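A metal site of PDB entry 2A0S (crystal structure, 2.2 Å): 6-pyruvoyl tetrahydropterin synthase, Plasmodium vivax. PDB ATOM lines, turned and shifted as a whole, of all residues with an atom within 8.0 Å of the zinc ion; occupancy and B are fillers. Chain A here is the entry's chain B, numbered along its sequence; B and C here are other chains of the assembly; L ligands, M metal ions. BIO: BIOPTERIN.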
ATOM      1  N   CYS A  34      -4.048  -4.647  -5.270  1.00  0.00           N
ATOM      2  CA  CYS A  34      -3.442  -4.131  -6.494  1.00  0.00           C
ATOM      3  C   CYS A  34      -2.298  -3.152  -6.280  1.00  0.00           C
ATOM      4  O   CYS A  34      -2.190  -2.531  -5.217  1.00  0.00           O
ATOM      5  CB  CYS A  34      -4.524  -3.451  -7.347  1.00  0.00           C
ATOM      6  SG  CYS A  34      -5.709  -4.592  -8.058  1.00  0.00           S
ATOM      7  N   ALA A  35      -1.455  -3.021  -7.300  1.00  0.00           N
ATOM      8  CA  ALA A  35      -0.430  -1.995  -7.348  1.00  0.00           C
ATOM      9  C   ALA A  35      -0.922  -0.836  -8.214  1.00  0.00           C
ATOM     10  O   ALA A  35      -1.715  -1.036  -9.136  1.00  0.00           O
ATOM     11  CB  ALA A  35       0.864  -2.564  -7.911  1.00  0.00           C
ATOM     12  N   HIS A  36      -0.457   0.371  -7.902  1.00  0.00           N
ATOM     13  CA  HIS A  36      -0.810   1.572  -8.670  1.00  0.00           C
ATOM     14  C   HIS A  36       0.072   2.758  -8.269  1.00  0.00           C
ATOM     15  O   HIS A  36       0.825   2.687  -7.302  1.00  0.00           O
ATOM     16  CB  HIS A  36      -2.303   1.915  -8.478  1.00  0.00           C
ATOM     17  CG  HIS A  36      -2.570   2.876  -7.350  1.00  0.00           C
ATOM     18  ND1 HIS A  36      -3.149   4.105  -7.543  1.00  0.00           N
ATOM     19  CD2 HIS A  36      -2.315   2.786  -6.023  1.00  0.00           C
ATOM     20  CE1 HIS A  36      -3.263   4.735  -6.386  1.00  0.00           C
ATOM     21  NE2 HIS A  36      -2.756   3.953  -5.443  1.00  0.00           N
ATOM     22  N   PHE A  37      -0.032   3.835  -9.043  1.00  0.00           N
ATOM     23  CA  PHE A  37       0.437   5.155  -8.617  1.00  0.00           C
ATOM     24  C   PHE A  37      -0.370   6.259  -9.283  1.00  0.00           C
ATOM     25  O   PHE A  37      -0.751   6.144 -10.454  1.00  0.00           O
ATOM     26  CB  PHE A  37       1.950   5.336  -8.824  1.00  0.00           C
ATOM     27  CG  PHE A  37       2.397   5.328 -10.262  1.00  0.00           C
ATOM     28  CD1 PHE A  37       2.469   6.513 -10.988  1.00  0.00           C
ATOM     29  CD2 PHE A  37       2.764   4.137 -10.881  1.00  0.00           C
ATOM     30  CE1 PHE A  37       2.887   6.511 -12.320  1.00  0.00           C
ATOM     31  CE2 PHE A  37       3.180   4.117 -12.211  1.00  0.00           C
ATOM     32  CZ  PHE A  37       3.253   5.309 -12.929  1.00  0.00           C
ATOM     33  N   ILE A  38      -0.649   7.312  -8.520  1.00  0.00           N
ATOM     34  CA  ILE A  38      -1.359   8.480  -9.050  1.00  0.00           C
ATOM     35  C   ILE A  38      -0.399   9.338  -9.859  1.00  0.00           C
ATOM     36  O   ILE A  38       0.723   9.602  -9.430  1.00  0.00           O
ATOM     37  CB  ILE A  38      -2.024   9.318  -7.924  1.00  0.00           C
ATOM     38  CG1 ILE A  38      -3.104   8.524  -7.189  1.00  0.00           C
ATOM     39  CG2 ILE A  38      -2.580  10.643  -8.461  1.00  0.00           C
ATOM     40  CD1 ILE A  38      -4.298   8.134  -8.050  1.00  0.00           C
ATOM     41  N   GLU A  45       3.504  10.186  -7.930  1.00  0.00           N
ATOM     42  CA  GLU A  45       3.929   9.468  -6.739  1.00  0.00           C
ATOM     43  C   GLU A  45       4.611   8.142  -7.091  1.00  0.00           C
ATOM     44  O   GLU A  45       4.500   7.666  -8.217  1.00  0.00           O
ATOM     45  CB  GLU A  45       2.748   9.239  -5.790  1.00  0.00           C
ATOM     46  CG  GLU A  45       1.678   8.304  -6.334  1.00  0.00           C
ATOM     47  CD  GLU A  45       0.420   8.313  -5.484  1.00  0.00           C
ATOM     48  OE1 GLU A  45       0.260   9.231  -4.651  1.00  0.00           O
ATOM     49  OE2 GLU A  45      -0.417   7.408  -5.657  1.00  0.00           O
ATOM     50  N   THR A  46       5.313   7.575  -6.116  1.00  0.00           N
ATOM     51  CA  THR A  46       6.023   6.324  -6.307  1.00  0.00           C
ATOM     52  C   THR A  46       5.078   5.125  -6.354  1.00  0.00           C
ATOM     53  O   THR A  46       3.966   5.183  -5.818  1.00  0.00           O
ATOM     54  CB  THR A  46       7.098   6.089  -5.221  1.00  0.00           C
ATOM     55  OG1 THR A  46       6.495   6.215  -3.929  1.00  0.00           O
ATOM     56  CG2 THR A  46       8.224   7.111  -5.342  1.00  0.00           C
ATOM     57  N   LEU A  47       5.510   4.056  -7.008  1.00  0.00           N
ATOM     58  CA  LEU A  47       4.753   2.813  -7.085  1.00  0.00           C
ATOM     59  C   LEU A  47       4.506   2.221  -5.705  1.00  0.00           C
ATOM     60  O   LEU A  47       5.439   2.081  -4.893  1.00  0.00           O
ATOM     61  CB  LEU A  47       5.480   1.797  -7.976  1.00  0.00           C
ATOM     62  CG  LEU A  47       4.868   0.394  -8.113  1.00  0.00           C
ATOM     63  CD1 LEU A  47       3.588   0.422  -8.939  1.00  0.00           C
ATOM     64  CD2 LEU A  47       5.867  -0.573  -8.722  1.00  0.00           C
ATOM     65  N   HIS A  48       3.254   1.900  -5.435  1.00  0.00           N
ATOM     66  CA  HIS A  48       2.859   1.239  -4.194  1.00  0.00           C
ATOM     67  C   HIS A  48       1.616   0.383  -4.456  1.00  0.00           C
ATOM     68  O   HIS A  48       1.312   0.078  -5.611  1.00  0.00           O
ATOM     69  CB  HIS A  48       2.620   2.254  -3.077  1.00  0.00           C
ATOM     70  CG  HIS A  48       1.513   3.218  -3.360  1.00  0.00           C
ATOM     71  ND1 HIS A  48       1.667   4.298  -4.200  1.00  0.00           N
ATOM     72  CD2 HIS A  48       0.247   3.286  -2.900  1.00  0.00           C
ATOM     73  CE1 HIS A  48       0.530   4.976  -4.264  1.00  0.00           C
ATOM     74  NE2 HIS A  48      -0.349   4.380  -3.483  1.00  0.00           N
ATOM     75  N   GLY A  49       0.909   0.012  -3.394  1.00  0.00           N
ATOM     76  CA  GLY A  49      -0.277  -0.825  -3.543  1.00  0.00           C
ATOM     77  C   GLY A  49      -1.267  -0.684  -2.404  1.00  0.00           C
ATOM     78  O   GLY A  49      -0.969  -0.022  -1.396  1.00  0.00           O
ATOM     79  N   HIS A  50      -2.433  -1.297  -2.568  1.00  0.00           N
ATOM     80  CA  HIS A  50      -3.503  -1.248  -1.583  1.00  0.00           C
ATOM     81  C   HIS A  50      -4.330  -2.531  -1.578  1.00  0.00           C
ATOM     82  O   HIS A  50      -4.413  -3.241  -2.576  1.00  0.00           O
ATOM     83  CB  HIS A  50      -4.452  -0.086  -1.870  1.00  0.00           C
ATOM     84  CG  HIS A  50      -3.810   1.263  -1.756  1.00  0.00           C
ATOM     85  ND1 HIS A  50      -3.591   1.883  -0.553  1.00  0.00           N
ATOM     86  CD2 HIS A  50      -3.348   2.110  -2.711  1.00  0.00           C
ATOM     87  CE1 HIS A  50      -3.009   3.058  -0.763  1.00  0.00           C
ATOM     88  NE2 HIS A  50      -2.857   3.214  -2.065  1.00  0.00           N
ATOM     89  N   TYR A  52      -7.790  -2.912  -1.795  1.00  0.00           N
ATOM     90  CA  TYR A  52      -9.026  -2.201  -2.121  1.00  0.00           C
ATOM     91  C   TYR A  52     -10.226  -3.022  -1.675  1.00  0.00           C
ATOM     92  O   TYR A  52     -10.191  -4.250  -1.718  1.00  0.00           O
ATOM     93  CB  TYR A  52      -9.127  -1.915  -3.613  1.00  0.00           C
ATOM     94  CG  TYR A  52      -8.177  -0.864  -4.149  1.00  0.00           C
ATOM     95  CD1 TYR A  52      -6.929  -1.215  -4.648  1.00  0.00           C
ATOM     96  CD2 TYR A  52      -8.545   0.482  -4.183  1.00  0.00           C
ATOM     97  CE1 TYR A  52      -6.054  -0.258  -5.160  1.00  0.00           C
ATOM     98  CE2 TYR A  52      -7.682   1.458  -4.697  1.00  0.00           C
ATOM     99  CZ  TYR A  52      -6.437   1.079  -5.185  1.00  0.00           C
ATOM    100  OH  TYR A  52      -5.578   2.028  -5.688  1.00  0.00           O
ATOM    101  N   SER A 132      -5.763   6.368 -11.643  1.00  0.00           N
ATOM    102  CA  SER A 132      -6.094   5.236 -10.780  1.00  0.00           C
ATOM    103  C   SER A 132      -6.486   5.708  -9.373  1.00  0.00           C
ATOM    104  O   SER A 132      -6.033   5.150  -8.371  1.00  0.00           O
ATOM    105  CB  SER A 132      -4.938   4.231 -10.734  1.00  0.00           C
ATOM    106  OG  SER A 132      -3.742   4.836 -10.269  1.00  0.00           O
ATOM    107  N   SER A 133      -7.327   6.740  -9.324  1.00  0.00           N
ATOM    108  CA  SER A 133      -7.839   7.266  -8.064  1.00  0.00           C
ATOM    109  C   SER A 133      -9.027   6.429  -7.591  1.00  0.00           C
ATOM    110  O   SER A 133      -9.673   5.741  -8.383  1.00  0.00           O
ATOM    111  CB  SER A 133      -8.256   8.726  -8.223  1.00  0.00           C
ATOM    112  OG  SER A 133      -9.389   8.859  -9.050  1.00  0.00           O
ATOM    113  N   THR A 134      -9.301   6.504  -6.297  1.00  0.00           N
ATOM    114  CA  THR A 134     -10.420   5.781  -5.690  1.00  0.00           C
ATOM    115  C   THR A 134     -11.756   6.209  -6.319  1.00  0.00           C
ATOM    116  O   THR A 134     -12.641   5.379  -6.542  1.00  0.00           O
ATOM    117  CB  THR A 134     -10.460   5.991  -4.161  1.00  0.00           C
ATOM    118  OG1 THR A 134      -9.121   6.005  -3.648  1.00  0.00           O
ATOM    119  CG2 THR A 134     -11.234   4.889  -3.487  1.00  0.00           C
ATOM    120  N   GLU A 168      -9.629   2.733  -0.593  1.00  0.00           N
ATOM    121  CA  GLU A 168      -8.207   2.558  -0.876  1.00  0.00           C
ATOM    122  C   GLU A 168      -7.552   1.984   0.380  1.00  0.00           C
ATOM    123  O   GLU A 168      -6.645   1.152   0.305  1.00  0.00           O
ATOM    124  CB  GLU A 168      -7.580   3.906  -1.218  1.00  0.00           C
ATOM    125  CG  GLU A 168      -6.337   3.838  -2.081  1.00  0.00           C
ATOM    126  CD  GLU A 168      -5.690   5.193  -2.297  1.00  0.00           C
ATOM    127  OE1 GLU A 168      -5.767   6.047  -1.386  1.00  0.00           O
ATOM    128  OE2 GLU A 168      -5.106   5.418  -3.378  1.00  0.00           O
ATOM    129  N   SER A 169      -8.028   2.446   1.532  1.00  0.00           N
ATOM    130  CA  SER A 169      -7.597   1.975   2.836  1.00  0.00           C
ATOM    131  C   SER A 169      -8.806   2.042   3.778  1.00  0.00           C
ATOM    132  O   SER A 169      -9.799   2.698   3.438  1.00  0.00           O
ATOM    133  CB  SER A 169      -6.450   2.828   3.365  1.00  0.00           C
ATOM    134  OG  SER A 169      -6.849   4.181   3.544  1.00  0.00           O
ATOM    135  N   GLN A 172      -9.638   5.763   3.937  1.00  0.00           N
ATOM    136  CA  GLN A 172      -9.981   6.579   2.759  1.00  0.00           C
ATOM    137  C   GLN A 172     -10.987   5.896   1.848  1.00  0.00           C
ATOM    138  O   GLN A 172     -10.696   4.845   1.257  1.00  0.00           O
ATOM    139  CB  GLN A 172      -8.703   6.928   1.976  1.00  0.00           C
ATOM    140  CG  GLN A 172      -7.702   7.787   2.743  1.00  0.00           C
ATOM    141  CD  GLN A 172      -6.384   7.945   2.021  1.00  0.00           C
ATOM    142  OE1 GLN A 172      -6.281   7.761   0.814  1.00  0.00           O
ATOM    143  NE2 GLN A 172      -5.342   8.305   2.775  1.00  0.00           N
ATOM    144  N   ASN B  33       1.740   1.020   2.804  1.00  0.00           N
ATOM    145  CA  ASN B  33       1.052   0.646   1.571  1.00  0.00           C
ATOM    146  C   ASN B  33       2.081   0.411   0.473  1.00  0.00           C
ATOM    147  O   ASN B  33       2.704   1.348  -0.025  1.00  0.00           O
ATOM    148  CB  ASN B  33       0.047   1.735   1.165  1.00  0.00           C
ATOM    149  CG  ASN B  33      -0.933   2.076   2.271  1.00  0.00           C
ATOM    150  OD1 ASN B  33      -1.161   1.285   3.194  1.00  0.00           O
ATOM    151  ND2 ASN B  33      -1.519   3.262   2.199  1.00  0.00           N
ATOM    152  N   ASN B  51      -2.219  -3.047   1.802  1.00  0.00           N
ATOM    153  CA  ASN B  51      -2.127  -2.177   2.966  1.00  0.00           C
ATOM    154  C   ASN B  51      -1.624  -3.020   4.126  1.00  0.00           C
ATOM    155  O   ASN B  51      -2.409  -3.674   4.815  1.00  0.00           O
ATOM    156  CB  ASN B  51      -3.484  -1.562   3.317  1.00  0.00           C
ATOM    157  CG  ASN B  51      -4.059  -0.718   2.189  1.00  0.00           C
ATOM    158  OD1 ASN B  51      -3.357   0.082   1.565  1.00  0.00           O
ATOM    159  ND2 ASN B  51      -5.355  -0.869   1.944  1.00  0.00           N
ATOM    160  N   HIS B  87       4.771   3.338   0.690  1.00  0.00           N
ATOM    161  CA  HIS B  87       4.764   3.892  -0.674  1.00  0.00           C
ATOM    162  C   HIS B  87       5.943   3.451  -1.545  1.00  0.00           C
ATOM    163  O   HIS B  87       6.512   4.264  -2.290  1.00  0.00           O
ATOM    164  CB  HIS B  87       4.615   5.412  -0.655  1.00  0.00           C
ATOM    165  CG  HIS B  87       3.200   5.887  -0.833  1.00  0.00           C
ATOM    166  ND1 HIS B  87       2.197   5.590   0.067  1.00  0.00           N
ATOM    167  CD2 HIS B  87       2.623   6.614  -1.815  1.00  0.00           C
ATOM    168  CE1 HIS B  87       1.071   6.131  -0.346  1.00  0.00           C
ATOM    169  NE2 HIS B  87       1.297   6.760  -1.488  1.00  0.00           N
ATOM    170  N   TYR C  67      -9.080  13.679  -8.421  1.00  0.00           N
ATOM    171  CA  TYR C  67      -9.601  13.844  -7.063  1.00  0.00           C
ATOM    172  C   TYR C  67     -10.786  14.787  -7.023  1.00  0.00           C
ATOM    173  O   TYR C  67     -10.879  15.711  -7.836  1.00  0.00           O
ATOM    174  CB  TYR C  67      -8.523  14.404  -6.128  1.00  0.00           C
ATOM    175  CG  TYR C  67      -7.255  13.582  -5.961  1.00  0.00           C
ATOM    176  CD1 TYR C  67      -7.244  12.200  -6.186  1.00  0.00           C
ATOM    177  CD2 TYR C  67      -6.079  14.189  -5.550  1.00  0.00           C
ATOM    178  CE1 TYR C  67      -6.073  11.460  -6.016  1.00  0.00           C
ATOM    179  CE2 TYR C  67      -4.908  13.456  -5.373  1.00  0.00           C
ATOM    180  CZ  TYR C  67      -4.914  12.098  -5.605  1.00  0.00           C
ATOM    181  OH  TYR C  67      -3.763  11.373  -5.433  1.00  0.00           O
HETATM  182  N1  BIO L   1      -7.312  11.771  -2.592  1.00  0.00           N
HETATM  183  N2  BIO L   1      -9.344  12.357  -3.516  1.00  0.00           N
HETATM  184  C2  BIO L   1      -8.392  11.452  -3.326  1.00  0.00           C
HETATM  185  N3  BIO L   1      -8.511  10.187  -3.915  1.00  0.00           N
HETATM  186  C4  BIO L   1      -7.492   9.247  -3.713  1.00  0.00           C
HETATM  187  O4  BIO L   1      -7.574   8.123  -4.217  1.00  0.00           O
HETATM  188  C4A BIO L   1      -6.387   9.602  -2.946  1.00  0.00           C
HETATM  189  C8A BIO L   1      -6.323  10.881  -2.392  1.00  0.00           C
HETATM  190  N8  BIO L   1      -5.267  11.233  -1.645  1.00  0.00           N
HETATM  191  C7  BIO L   1      -4.274  10.380  -1.425  1.00  0.00           C
HETATM  192  C6  BIO L   1      -4.331   9.095  -1.974  1.00  0.00           C
HETATM  193  N5  BIO L   1      -5.382   8.730  -2.723  1.00  0.00           N
HETATM  194  C9  BIO L   1      -3.194   8.081  -1.730  1.00  0.00           C
HETATM  195  O9  BIO L   1      -2.962   7.934  -0.321  1.00  0.00           O
HETATM  196  C10 BIO L   1      -1.917   8.493  -2.475  1.00  0.00           C
HETATM  197  O10 BIO L   1      -1.286   7.318  -2.985  1.00  0.00           O
HETATM  198  C11 BIO L   1      -0.953   9.295  -1.586  1.00  0.00           C
HETATM  199 ZN    ZN M   1      -2.502   4.792  -3.415  1.00  0.00          ZN
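The zinc ion is bound by NE2 of His 50, NE2 of His 48 and NE2 of His 36.
The zinc ion has three donor atoms within binding distance.
Slightly farther from the zinc ion lies OE2 of Glu 168 (2.7 Å).
Slightly farther from the zinc ion lies O10 of the ligand (2.8 Å).
Within 4 Å of the zinc ion: His 36, His 48, His 50 and Glu 168.
An oxygen (O10) of the ligand lies close to a ring nitrogen (NE2) of His 48 (3.1 Å).
The side-chain carboxylate (OE1) of Glu 168 sits close to a nitrogen (N5) of the ligand (3.0 Å).
OE2 of Glu 45 lies within hydrogen-bond range of O10 of the ligand (2.8 Å).
O10 of the ligand lies within hydrogen-bond range of NE2 of His 87 of chain B (3.0 Å).
The backbone NH (N) of Thr 134 is in hydrogen-bond range of an oxygen (O4) of the ligand (3.2 Å).
The side-chain hydroxyl (OG1) of Thr 134 sits at hydrogen-bond distance from an oxygen (O4) of the ligand.
The backbone carbonyl oxygen (O) of Glu 168 lies within hydrogen-bond range of a ring nitrogen (ND1) of His 50 (3.3 Å).
A ring nitrogen (ND1) of His 50 lies within hydrogen-bond range of the side-chain amide oxygen of Asn 51 of chain B, at 2.8 Å.
The backbone carbonyl oxygen (O) of Cys 34 lies within hydrogen-bond range of the backbone NH (N) of His 50 (2.9 Å).
O of Thr 46 sits at hydrogen-bond distance from ND1 of His 48 (2.9 Å).
A ring nitrogen (NE2) of His 36 sits close to the side-chain carboxylate (OE2) of Glu 168 (3.5 Å).
NE2 of His 36 sits close to OH of Tyr 52 (3.4 Å).
A ring nitrogen (ND1) of His 36 lies within hydrogen-bond range of the side-chain hydroxyl (OG) of Ser 132 (2.9 Å).
O of Glu 168 is in hydrogen-bond range of ND2 of Asn 51 of chain B.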
